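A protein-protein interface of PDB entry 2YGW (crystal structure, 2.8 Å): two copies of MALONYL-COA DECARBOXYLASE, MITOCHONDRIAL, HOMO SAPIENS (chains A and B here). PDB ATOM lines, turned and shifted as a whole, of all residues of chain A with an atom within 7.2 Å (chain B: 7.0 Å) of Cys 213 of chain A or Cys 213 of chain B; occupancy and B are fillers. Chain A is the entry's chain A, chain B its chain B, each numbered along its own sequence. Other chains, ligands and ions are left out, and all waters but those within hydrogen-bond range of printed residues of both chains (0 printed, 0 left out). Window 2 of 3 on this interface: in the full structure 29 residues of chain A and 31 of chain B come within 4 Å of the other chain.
SG of Cys 213 of chain A is in hydrogen-bond range of OG of Ser 214 of chain B (3.5 Å).
O of Phe 164 of chain A sits at hydrogen-bond distance from N of Cys 213 of chain A (2.7 Å). SG of Cys 213 of chain A lies within hydrogen-bond range of OD1 of Asn 166 of chain A, at 3.4 Å. The backbone NH (N) of Ser 214 of chain A sits close to a ring nitrogen (ND1) of His 212 of chain A. The backbone carbonyl oxygen of Phe 164 of chain B is in hydrogen-bond range of the backbone NH of Cys 213 of chain B (2.9 Å). The side-chain amide oxygen of Asn 166 of chain B lies within hydrogen-bond range of the side-chain sulfur of Cys 213 of chain B (3.3 Å). ND1 of His 212 of chain B lies close to N of Ser 214 of chain B, 3.2 Å away.
Among the printed residues, pairs that only touch across the chains: Trp 159 of chain A with Phe 164 of chain B, Phe 164 of chain A with Trp 159 of chain B, Phe 164 of chain A with Phe 164 of chain B, Phe 164 of chain A with His 212 of chain B, Phe 164 of chain A with Ser 214 of chain B, His 212 of chain A with Phe 164 of chain B, Cys 213 of chain A with Cys 213 of chain B, Ser 214 of chain A with Gly 163 of chain B and Ser 214 of chain A with Cys 213 of chain B.
Of the printed residues of chain B, Trp 159 of chain A touches Phe 164 (3.6 Å). Of the printed residues of chain B, Cys 213 of chain A touches Cys 213 and Ser 214. Of the printed residues of chain B, Ser 214 of chain A touches Gly 163 and Cys 213. Pro 216 of chain A touches none of the printed residues of chain B. Of the printed residues of chain A, Gly 163 of chain B touches Ser 214. Printed residues of chain A within 4 Å of Phe 164 of chain B: Trp 159, Phe 164 and His 212. Of the printed residues of chain A, His 212 of chain B touches Phe 164 (3.5 Å). Of the printed residues of chain A, Cys 213 of chain B touches Cys 213 (3.7 Å) and Ser 214 (3.8 Å). The nearest printed residue of chain B that does not touch Cys 213 of chain A is Asn 166 of chain B (5.7 Å). The nearest printed residue of chain B that does not touch Trp 159 of chain A is Trp 159 of chain B (5.9 Å).
Of the 13 printed residues of chain B, 6 touch a printed residue of chain A. Hydrophobic or aromatic side chains of chain B within 4 Å of the printed part of chain A: Trp 159, Phe 164 and His 212. Hydrophobic or aromatic side chains of chain A within 4 Å of the printed part of chain B: Phe 164 and His 212.
Trp 159 of chain A touches Phe 164 of chain B, and with the chains exchanged Phe 164 of chain A touches Trp 159 of chain B. Phe 164 of chain A touches His 212 of chain B, and with the chains exchanged His 212 of chain A touches Phe 164 of chain B. Cys 213 of chain B touches its own counterpart, Cys 213 of chain A. Ser 214 of chain A touches Gly 163 of chain B, but with the chains exchanged Gly 163 of chain A does not touch Ser 214 of chain B (4.1 Å). 13 positions are printed for both chains. Of the 10 pairs that touch across the chains among the printed residues, 8 have their exchanged pair printed and touching as well.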
ATOM      1  N   TRP A 159     -10.099 -17.133   5.039  1.00  0.00           N
ATOM      2  CA  TRP A 159      -9.771 -16.586   3.718  1.00  0.00           C
ATOM      3  C   TRP A 159      -8.649 -15.552   3.812  1.00  0.00           C
ATOM      4  O   TRP A 159      -7.880 -15.430   2.874  1.00  0.00           O
ATOM      5  CB  TRP A 159     -11.012 -15.992   3.016  1.00  0.00           C
ATOM      6  CG  TRP A 159     -12.126 -16.977   2.779  1.00  0.00           C
ATOM      7  CD1 TRP A 159     -11.998 -18.288   2.435  1.00  0.00           C
ATOM      8  CD2 TRP A 159     -13.547 -16.718   2.851  1.00  0.00           C
ATOM      9  NE1 TRP A 159     -13.244 -18.879   2.337  1.00  0.00           N
ATOM     10  CE2 TRP A 159     -14.214 -17.931   2.561  1.00  0.00           C
ATOM     11  CE3 TRP A 159     -14.321 -15.572   3.095  1.00  0.00           C
ATOM     12  CZ2 TRP A 159     -15.627 -18.031   2.518  1.00  0.00           C
ATOM     13  CZ3 TRP A 159     -15.710 -15.667   3.040  1.00  0.00           C
ATOM     14  CH2 TRP A 159     -16.351 -16.887   2.769  1.00  0.00           C
ATOM     15  N   SER A 162      -2.730 -15.237   7.586  1.00  0.00           N
ATOM     16  CA  SER A 162      -1.361 -14.749   7.400  1.00  0.00           C
ATOM     17  C   SER A 162      -0.733 -15.226   6.081  1.00  0.00           C
ATOM     18  O   SER A 162      -0.198 -14.403   5.353  1.00  0.00           O
ATOM     19  CB  SER A 162      -0.497 -15.175   8.584  1.00  0.00           C
ATOM     20  OG  SER A 162       0.789 -14.580   8.539  1.00  0.00           O
ATOM     21  N   GLY A 163      -0.864 -16.513   5.762  1.00  0.00           N
ATOM     22  CA  GLY A 163      -0.348 -17.114   4.542  1.00  0.00           C
ATOM     23  C   GLY A 163      -1.046 -16.745   3.238  1.00  0.00           C
ATOM     24  O   GLY A 163      -0.684 -17.276   2.184  1.00  0.00           O
ATOM     25  N   PHE A 164      -2.049 -15.865   3.261  1.00  0.00           N
ATOM     26  CA  PHE A 164      -2.702 -15.453   2.017  1.00  0.00           C
ATOM     27  C   PHE A 164      -2.525 -13.970   1.797  1.00  0.00           C
ATOM     28  O   PHE A 164      -3.005 -13.435   0.810  1.00  0.00           O
ATOM     29  CB  PHE A 164      -4.175 -15.867   1.993  1.00  0.00           C
ATOM     30  CG  PHE A 164      -4.264 -17.365   1.916  1.00  0.00           C
ATOM     31  CD1 PHE A 164      -3.868 -18.041   0.763  1.00  0.00           C
ATOM     32  CD2 PHE A 164      -4.602 -18.113   3.038  1.00  0.00           C
ATOM     33  CE1 PHE A 164      -3.874 -19.438   0.713  1.00  0.00           C
ATOM     34  CE2 PHE A 164      -4.597 -19.515   2.995  1.00  0.00           C
ATOM     35  CZ  PHE A 164      -4.242 -20.166   1.829  1.00  0.00           C
ATOM     36  N   LEU A 165      -1.758 -13.326   2.684  1.00  0.00           N
ATOM     37  CA  LEU A 165      -1.449 -11.899   2.694  1.00  0.00           C
ATOM     38  C   LEU A 165      -0.020 -11.638   2.246  1.00  0.00           C
ATOM     39  O   LEU A 165       0.876 -12.376   2.641  1.00  0.00           O
ATOM     40  CB  LEU A 165      -1.658 -11.325   4.108  1.00  0.00           C
ATOM     41  CG  LEU A 165      -2.969 -11.660   4.815  1.00  0.00           C
ATOM     42  CD1 LEU A 165      -2.865 -11.373   6.270  1.00  0.00           C
ATOM     43  CD2 LEU A 165      -4.133 -10.898   4.243  1.00  0.00           C
ATOM     44  N   ASN A 166       0.195 -10.593   1.423  1.00  0.00           N
ATOM     45  CA  ASN A 166       1.522 -10.177   0.951  1.00  0.00           C
ATOM     46  C   ASN A 166       1.936  -8.900   1.673  1.00  0.00           C
ATOM     47  O   ASN A 166       1.091  -8.025   1.868  1.00  0.00           O
ATOM     48  CB  ASN A 166       1.531  -9.932  -0.565  1.00  0.00           C
ATOM     49  CG  ASN A 166       1.306 -11.146  -1.452  1.00  0.00           C
ATOM     50  OD1 ASN A 166       1.903 -12.227  -1.274  1.00  0.00           O
ATOM     51  ND2 ASN A 166       0.469 -10.966  -2.473  1.00  0.00           N
ATOM     52  N   SER A 211      -1.700  -6.869   1.653  1.00  0.00           N
ATOM     53  CA  SER A 211      -2.714  -7.043   0.624  1.00  0.00           C
ATOM     54  C   SER A 211      -3.027  -8.538   0.527  1.00  0.00           C
ATOM     55  O   SER A 211      -2.180  -9.366   0.894  1.00  0.00           O
ATOM     56  CB  SER A 211      -2.241  -6.481  -0.710  1.00  0.00           C
ATOM     57  OG  SER A 211      -1.226  -7.281  -1.297  1.00  0.00           O
ATOM     58  N   HIS A 212      -4.221  -8.906   0.060  1.00  0.00           N
ATOM     59  CA  HIS A 212      -4.519 -10.337  -0.092  1.00  0.00           C
ATOM     60  C   HIS A 212      -3.811 -10.790  -1.383  1.00  0.00           C
ATOM     61  O   HIS A 212      -3.696  -9.969  -2.301  1.00  0.00           O
ATOM     62  CB  HIS A 212      -6.056 -10.580  -0.119  1.00  0.00           C
ATOM     63  CG  HIS A 212      -6.458 -12.015   0.045  1.00  0.00           C
ATOM     64  ND1 HIS A 212      -6.396 -12.903  -1.005  1.00  0.00           N
ATOM     65  CD2 HIS A 212      -6.929 -12.664   1.130  1.00  0.00           C
ATOM     66  CE1 HIS A 212      -6.800 -14.066  -0.528  1.00  0.00           C
ATOM     67  NE2 HIS A 212      -7.151 -13.971   0.743  1.00  0.00           N
ATOM     68  N   CYS A 213      -3.321 -12.058  -1.463  1.00  0.00           N
ATOM     69  CA  CYS A 213      -2.646 -12.576  -2.664  1.00  0.00           C
ATOM     70  C   CYS A 213      -3.535 -12.366  -3.910  1.00  0.00           C
ATOM     71  O   CYS A 213      -3.018 -12.171  -5.008  1.00  0.00           O
ATOM     72  CB  CYS A 213      -2.260 -14.050  -2.496  1.00  0.00           C
ATOM     73  SG  CYS A 213      -0.761 -14.347  -1.509  1.00  0.00           S
ATOM     74  N   SER A 214      -4.875 -12.393  -3.725  1.00  0.00           N
ATOM     75  CA  SER A 214      -5.895 -12.234  -4.767  1.00  0.00           C
ATOM     76  C   SER A 214      -5.964 -10.805  -5.300  1.00  0.00           C
ATOM     77  O   SER A 214      -6.161 -10.608  -6.500  1.00  0.00           O
ATOM     78  CB  SER A 214      -7.264 -12.644  -4.236  1.00  0.00           C
ATOM     79  OG  SER A 214      -7.272 -14.022  -3.910  1.00  0.00           O
ATOM     80  N   THR A 215      -5.815  -9.810  -4.407  1.00  0.00           N
ATOM     81  CA  THR A 215      -5.912  -8.382  -4.729  1.00  0.00           C
ATOM     82  C   THR A 215      -4.599  -7.644  -4.372  1.00  0.00           C
ATOM     83  O   THR A 215      -4.517  -7.019  -3.311  1.00  0.00           O
ATOM     84  CB  THR A 215      -7.116  -7.759  -3.999  1.00  0.00           C
ATOM     85  OG1 THR A 215      -6.986  -8.015  -2.598  1.00  0.00           O
ATOM     86  CG2 THR A 215      -8.446  -8.296  -4.493  1.00  0.00           C
ATOM     87  N   PRO A 216      -3.566  -7.683  -5.247  1.00  0.00           N
ATOM     88  CA  PRO A 216      -2.331  -6.932  -4.950  1.00  0.00           C
ATOM     89  C   PRO A 216      -2.552  -5.414  -5.076  1.00  0.00           C
ATOM     90  O   PRO A 216      -3.367  -4.974  -5.905  1.00  0.00           O
ATOM     91  CB  PRO A 216      -1.348  -7.439  -6.015  1.00  0.00           C
ATOM     92  CG  PRO A 216      -2.033  -8.634  -6.679  1.00  0.00           C
ATOM     93  CD  PRO A 216      -3.478  -8.347  -6.564  1.00  0.00           C
ATOM     94  N   LEU A 220      -5.241  -3.651   3.366  1.00  0.00           N
ATOM     95  CA  LEU A 220      -6.185  -4.268   4.300  1.00  0.00           C
ATOM     96  C   LEU A 220      -5.927  -3.760   5.721  1.00  0.00           C
ATOM     97  O   LEU A 220      -6.855  -3.681   6.511  1.00  0.00           O
ATOM     98  CB  LEU A 220      -6.069  -5.806   4.272  1.00  0.00           C
ATOM     99  CG  LEU A 220      -6.337  -6.516   2.954  1.00  0.00           C
ATOM    100  CD1 LEU A 220      -5.809  -7.888   2.998  1.00  0.00           C
ATOM    101  CD2 LEU A 220      -7.814  -6.620   2.668  1.00  0.00           C
ATOM    102  N   TRP B 159      -9.131 -23.005  -0.149  1.00  0.00           N
ATOM    103  CA  TRP B 159      -7.908 -22.309  -0.572  1.00  0.00           C
ATOM    104  C   TRP B 159      -7.712 -22.349  -2.077  1.00  0.00           C
ATOM    105  O   TRP B 159      -7.090 -21.453  -2.611  1.00  0.00           O
ATOM    106  CB  TRP B 159      -6.668 -22.909   0.125  1.00  0.00           C
ATOM    107  CG  TRP B 159      -6.693 -22.775   1.622  1.00  0.00           C
ATOM    108  CD1 TRP B 159      -7.221 -21.738   2.349  1.00  0.00           C
ATOM    109  CD2 TRP B 159      -6.139 -23.689   2.573  1.00  0.00           C
ATOM    110  NE1 TRP B 159      -7.060 -21.972   3.692  1.00  0.00           N
ATOM    111  CE2 TRP B 159      -6.372 -23.148   3.857  1.00  0.00           C
ATOM    112  CE3 TRP B 159      -5.443 -24.904   2.465  1.00  0.00           C
ATOM    113  CZ2 TRP B 159      -5.935 -23.774   5.019  1.00  0.00           C
ATOM    114  CZ3 TRP B 159      -5.035 -25.543   3.626  1.00  0.00           C
ATOM    115  CH2 TRP B 159      -5.278 -24.974   4.883  1.00  0.00           C
ATOM    116  N   SER B 162     -12.207 -21.109  -7.044  1.00  0.00           N
ATOM    117  CA  SER B 162     -11.979 -20.303  -8.263  1.00  0.00           C
ATOM    118  C   SER B 162     -11.448 -18.870  -7.961  1.00  0.00           C
ATOM    119  O   SER B 162     -10.489 -18.441  -8.593  1.00  0.00           O
ATOM    120  CB  SER B 162     -13.242 -20.233  -9.112  1.00  0.00           C
ATOM    121  OG  SER B 162     -12.928 -20.220 -10.493  1.00  0.00           O
ATOM    122  N   GLY B 163     -12.006 -18.207  -6.951  1.00  0.00           N
ATOM    123  CA  GLY B 163     -11.613 -16.867  -6.534  1.00  0.00           C
ATOM    124  C   GLY B 163     -10.158 -16.703  -6.152  1.00  0.00           C
ATOM    125  O   GLY B 163      -9.600 -15.609  -6.274  1.00  0.00           O
ATOM    126  N   PHE B 164      -9.539 -17.787  -5.675  1.00  0.00           N
ATOM    127  CA  PHE B 164      -8.137 -17.834  -5.260  1.00  0.00           C
ATOM    128  C   PHE B 164      -7.196 -18.310  -6.411  1.00  0.00           C
ATOM    129  O   PHE B 164      -5.978 -18.414  -6.212  1.00  0.00           O
ATOM    130  CB  PHE B 164      -7.998 -18.798  -4.078  1.00  0.00           C
ATOM    131  CG  PHE B 164      -8.134 -18.295  -2.655  1.00  0.00           C
ATOM    132  CD1 PHE B 164      -9.391 -18.169  -2.060  1.00  0.00           C
ATOM    133  CD2 PHE B 164      -7.004 -18.113  -1.852  1.00  0.00           C
ATOM    134  CE1 PHE B 164      -9.515 -17.796  -0.718  1.00  0.00           C
ATOM    135  CE2 PHE B 164      -7.130 -17.752  -0.504  1.00  0.00           C
ATOM    136  CZ  PHE B 164      -8.385 -17.602   0.054  1.00  0.00           C
ATOM    137  N   LEU B 165      -7.759 -18.640  -7.594  1.00  0.00           N
ATOM    138  CA  LEU B 165      -6.955 -19.123  -8.719  1.00  0.00           C
ATOM    139  C   LEU B 165      -6.832 -18.062  -9.789  1.00  0.00           C
ATOM    140  O   LEU B 165      -7.791 -17.309  -9.987  1.00  0.00           O
ATOM    141  CB  LEU B 165      -7.582 -20.396  -9.335  1.00  0.00           C
ATOM    142  CG  LEU B 165      -7.938 -21.576  -8.408  1.00  0.00           C
ATOM    143  CD1 LEU B 165      -8.721 -22.603  -9.145  1.00  0.00           C
ATOM    144  CD2 LEU B 165      -6.703 -22.200  -7.752  1.00  0.00           C
ATOM    145  N   ASN B 166      -5.650 -17.995 -10.484  1.00  0.00           N
ATOM    146  CA  ASN B 166      -5.419 -17.116 -11.652  1.00  0.00           C
ATOM    147  C   ASN B 166      -5.525 -17.925 -12.963  1.00  0.00           C
ATOM    148  O   ASN B 166      -5.003 -19.045 -13.021  1.00  0.00           O
ATOM    149  CB  ASN B 166      -4.035 -16.432 -11.655  1.00  0.00           C
ATOM    150  CG  ASN B 166      -3.507 -15.751 -10.421  1.00  0.00           C
ATOM    151  OD1 ASN B 166      -3.974 -14.665 -10.015  1.00  0.00           O
ATOM    152  ND2 ASN B 166      -2.360 -16.267  -9.950  1.00  0.00           N
ATOM    153  N   SER B 211      -3.073 -21.213 -11.757  1.00  0.00           N
ATOM    154  CA  SER B 211      -2.044 -21.186 -10.728  1.00  0.00           C
ATOM    155  C   SER B 211      -2.695 -20.621  -9.474  1.00  0.00           C
ATOM    156  O   SER B 211      -3.705 -19.909  -9.588  1.00  0.00           O
ATOM    157  CB  SER B 211      -0.829 -20.381 -11.175  1.00  0.00           C
ATOM    158  OG  SER B 211      -1.156 -19.046 -11.531  1.00  0.00           O
ATOM    159  N   HIS B 212      -2.189 -20.966  -8.287  1.00  0.00           N
ATOM    160  CA  HIS B 212      -2.747 -20.390  -7.066  1.00  0.00           C
ATOM    161  C   HIS B 212      -2.244 -18.914  -6.971  1.00  0.00           C
ATOM    162  O   HIS B 212      -1.100 -18.650  -7.360  1.00  0.00           O
ATOM    163  CB  HIS B 212      -2.379 -21.243  -5.839  1.00  0.00           C
ATOM    164  CG  HIS B 212      -3.133 -20.849  -4.619  1.00  0.00           C
ATOM    165  ND1 HIS B 212      -2.603 -19.970  -3.706  1.00  0.00           N
ATOM    166  CD2 HIS B 212      -4.391 -21.161  -4.243  1.00  0.00           C
ATOM    167  CE1 HIS B 212      -3.534 -19.797  -2.784  1.00  0.00           C
ATOM    168  NE2 HIS B 212      -4.629 -20.491  -3.064  1.00  0.00           N
ATOM    169  N   CYS B 213      -3.090 -17.952  -6.503  1.00  0.00           N
ATOM    170  CA  CYS B 213      -2.716 -16.531  -6.400  1.00  0.00           C
ATOM    171  C   CYS B 213      -1.392 -16.347  -5.628  1.00  0.00           C
ATOM    172  O   CYS B 213      -0.650 -15.400  -5.891  1.00  0.00           O
ATOM    173  CB  CYS B 213      -3.843 -15.719  -5.771  1.00  0.00           C
ATOM    174  SG  CYS B 213      -5.140 -15.235  -6.940  1.00  0.00           S
ATOM    175  N   SER B 214      -1.086 -17.280  -4.706  1.00  0.00           N
ATOM    176  CA  SER B 214       0.130 -17.276  -3.887  1.00  0.00           C
ATOM    177  C   SER B 214       1.379 -17.648  -4.694  1.00  0.00           C
ATOM    178  O   SER B 214       2.448 -17.088  -4.454  1.00  0.00           O
ATOM    179  CB  SER B 214      -0.021 -18.240  -2.713  1.00  0.00           C
ATOM    180  OG  SER B 214      -1.040 -17.776  -1.843  1.00  0.00           O
ATOM    181  N   THR B 215       1.236 -18.600  -5.643  1.00  0.00           N
ATOM    182  CA  THR B 215       2.312 -19.120  -6.494  1.00  0.00           C
ATOM    183  C   THR B 215       2.015 -18.867  -7.992  1.00  0.00           C
ATOM    184  O   THR B 215       1.532 -19.774  -8.679  1.00  0.00           O
ATOM    185  CB  THR B 215       2.529 -20.609  -6.218  1.00  0.00           C
ATOM    186  OG1 THR B 215       1.292 -21.287  -6.411  1.00  0.00           O
ATOM    187  CG2 THR B 215       3.072 -20.880  -4.824  1.00  0.00           C
ATOM    188  N   PRO B 216       2.284 -17.653  -8.526  1.00  0.00           N
ATOM    189  CA  PRO B 216       2.031 -17.412  -9.958  1.00  0.00           C
ATOM    190  C   PRO B 216       3.024 -18.179 -10.836  1.00  0.00           C
ATOM    191  O   PRO B 216       4.175 -18.369 -10.436  1.00  0.00           O
ATOM    192  CB  PRO B 216       2.212 -15.887 -10.095  1.00  0.00           C
ATOM    193  CG  PRO B 216       2.228 -15.346  -8.691  1.00  0.00           C
ATOM    194  CD  PRO B 216       2.845 -16.447  -7.888  1.00  0.00           C
ATOM    195  N   LEU B 220      -1.564 -25.897 -11.767  1.00  0.00           N
ATOM    196  CA  LEU B 220      -2.364 -26.844 -10.977  1.00  0.00           C
ATOM    197  C   LEU B 220      -3.194 -27.738 -11.881  1.00  0.00           C
ATOM    198  O   LEU B 220      -3.458 -28.884 -11.524  1.00  0.00           O
ATOM    199  CB  LEU B 220      -3.321 -26.094 -10.018  1.00  0.00           C
ATOM    200  CG  LEU B 220      -2.731 -25.275  -8.902  1.00  0.00           C
ATOM    201  CD1 LEU B 220      -3.776 -24.433  -8.298  1.00  0.00           C
ATOM    202  CD2 LEU B 220      -2.148 -26.164  -7.827  1.00  0.00           C
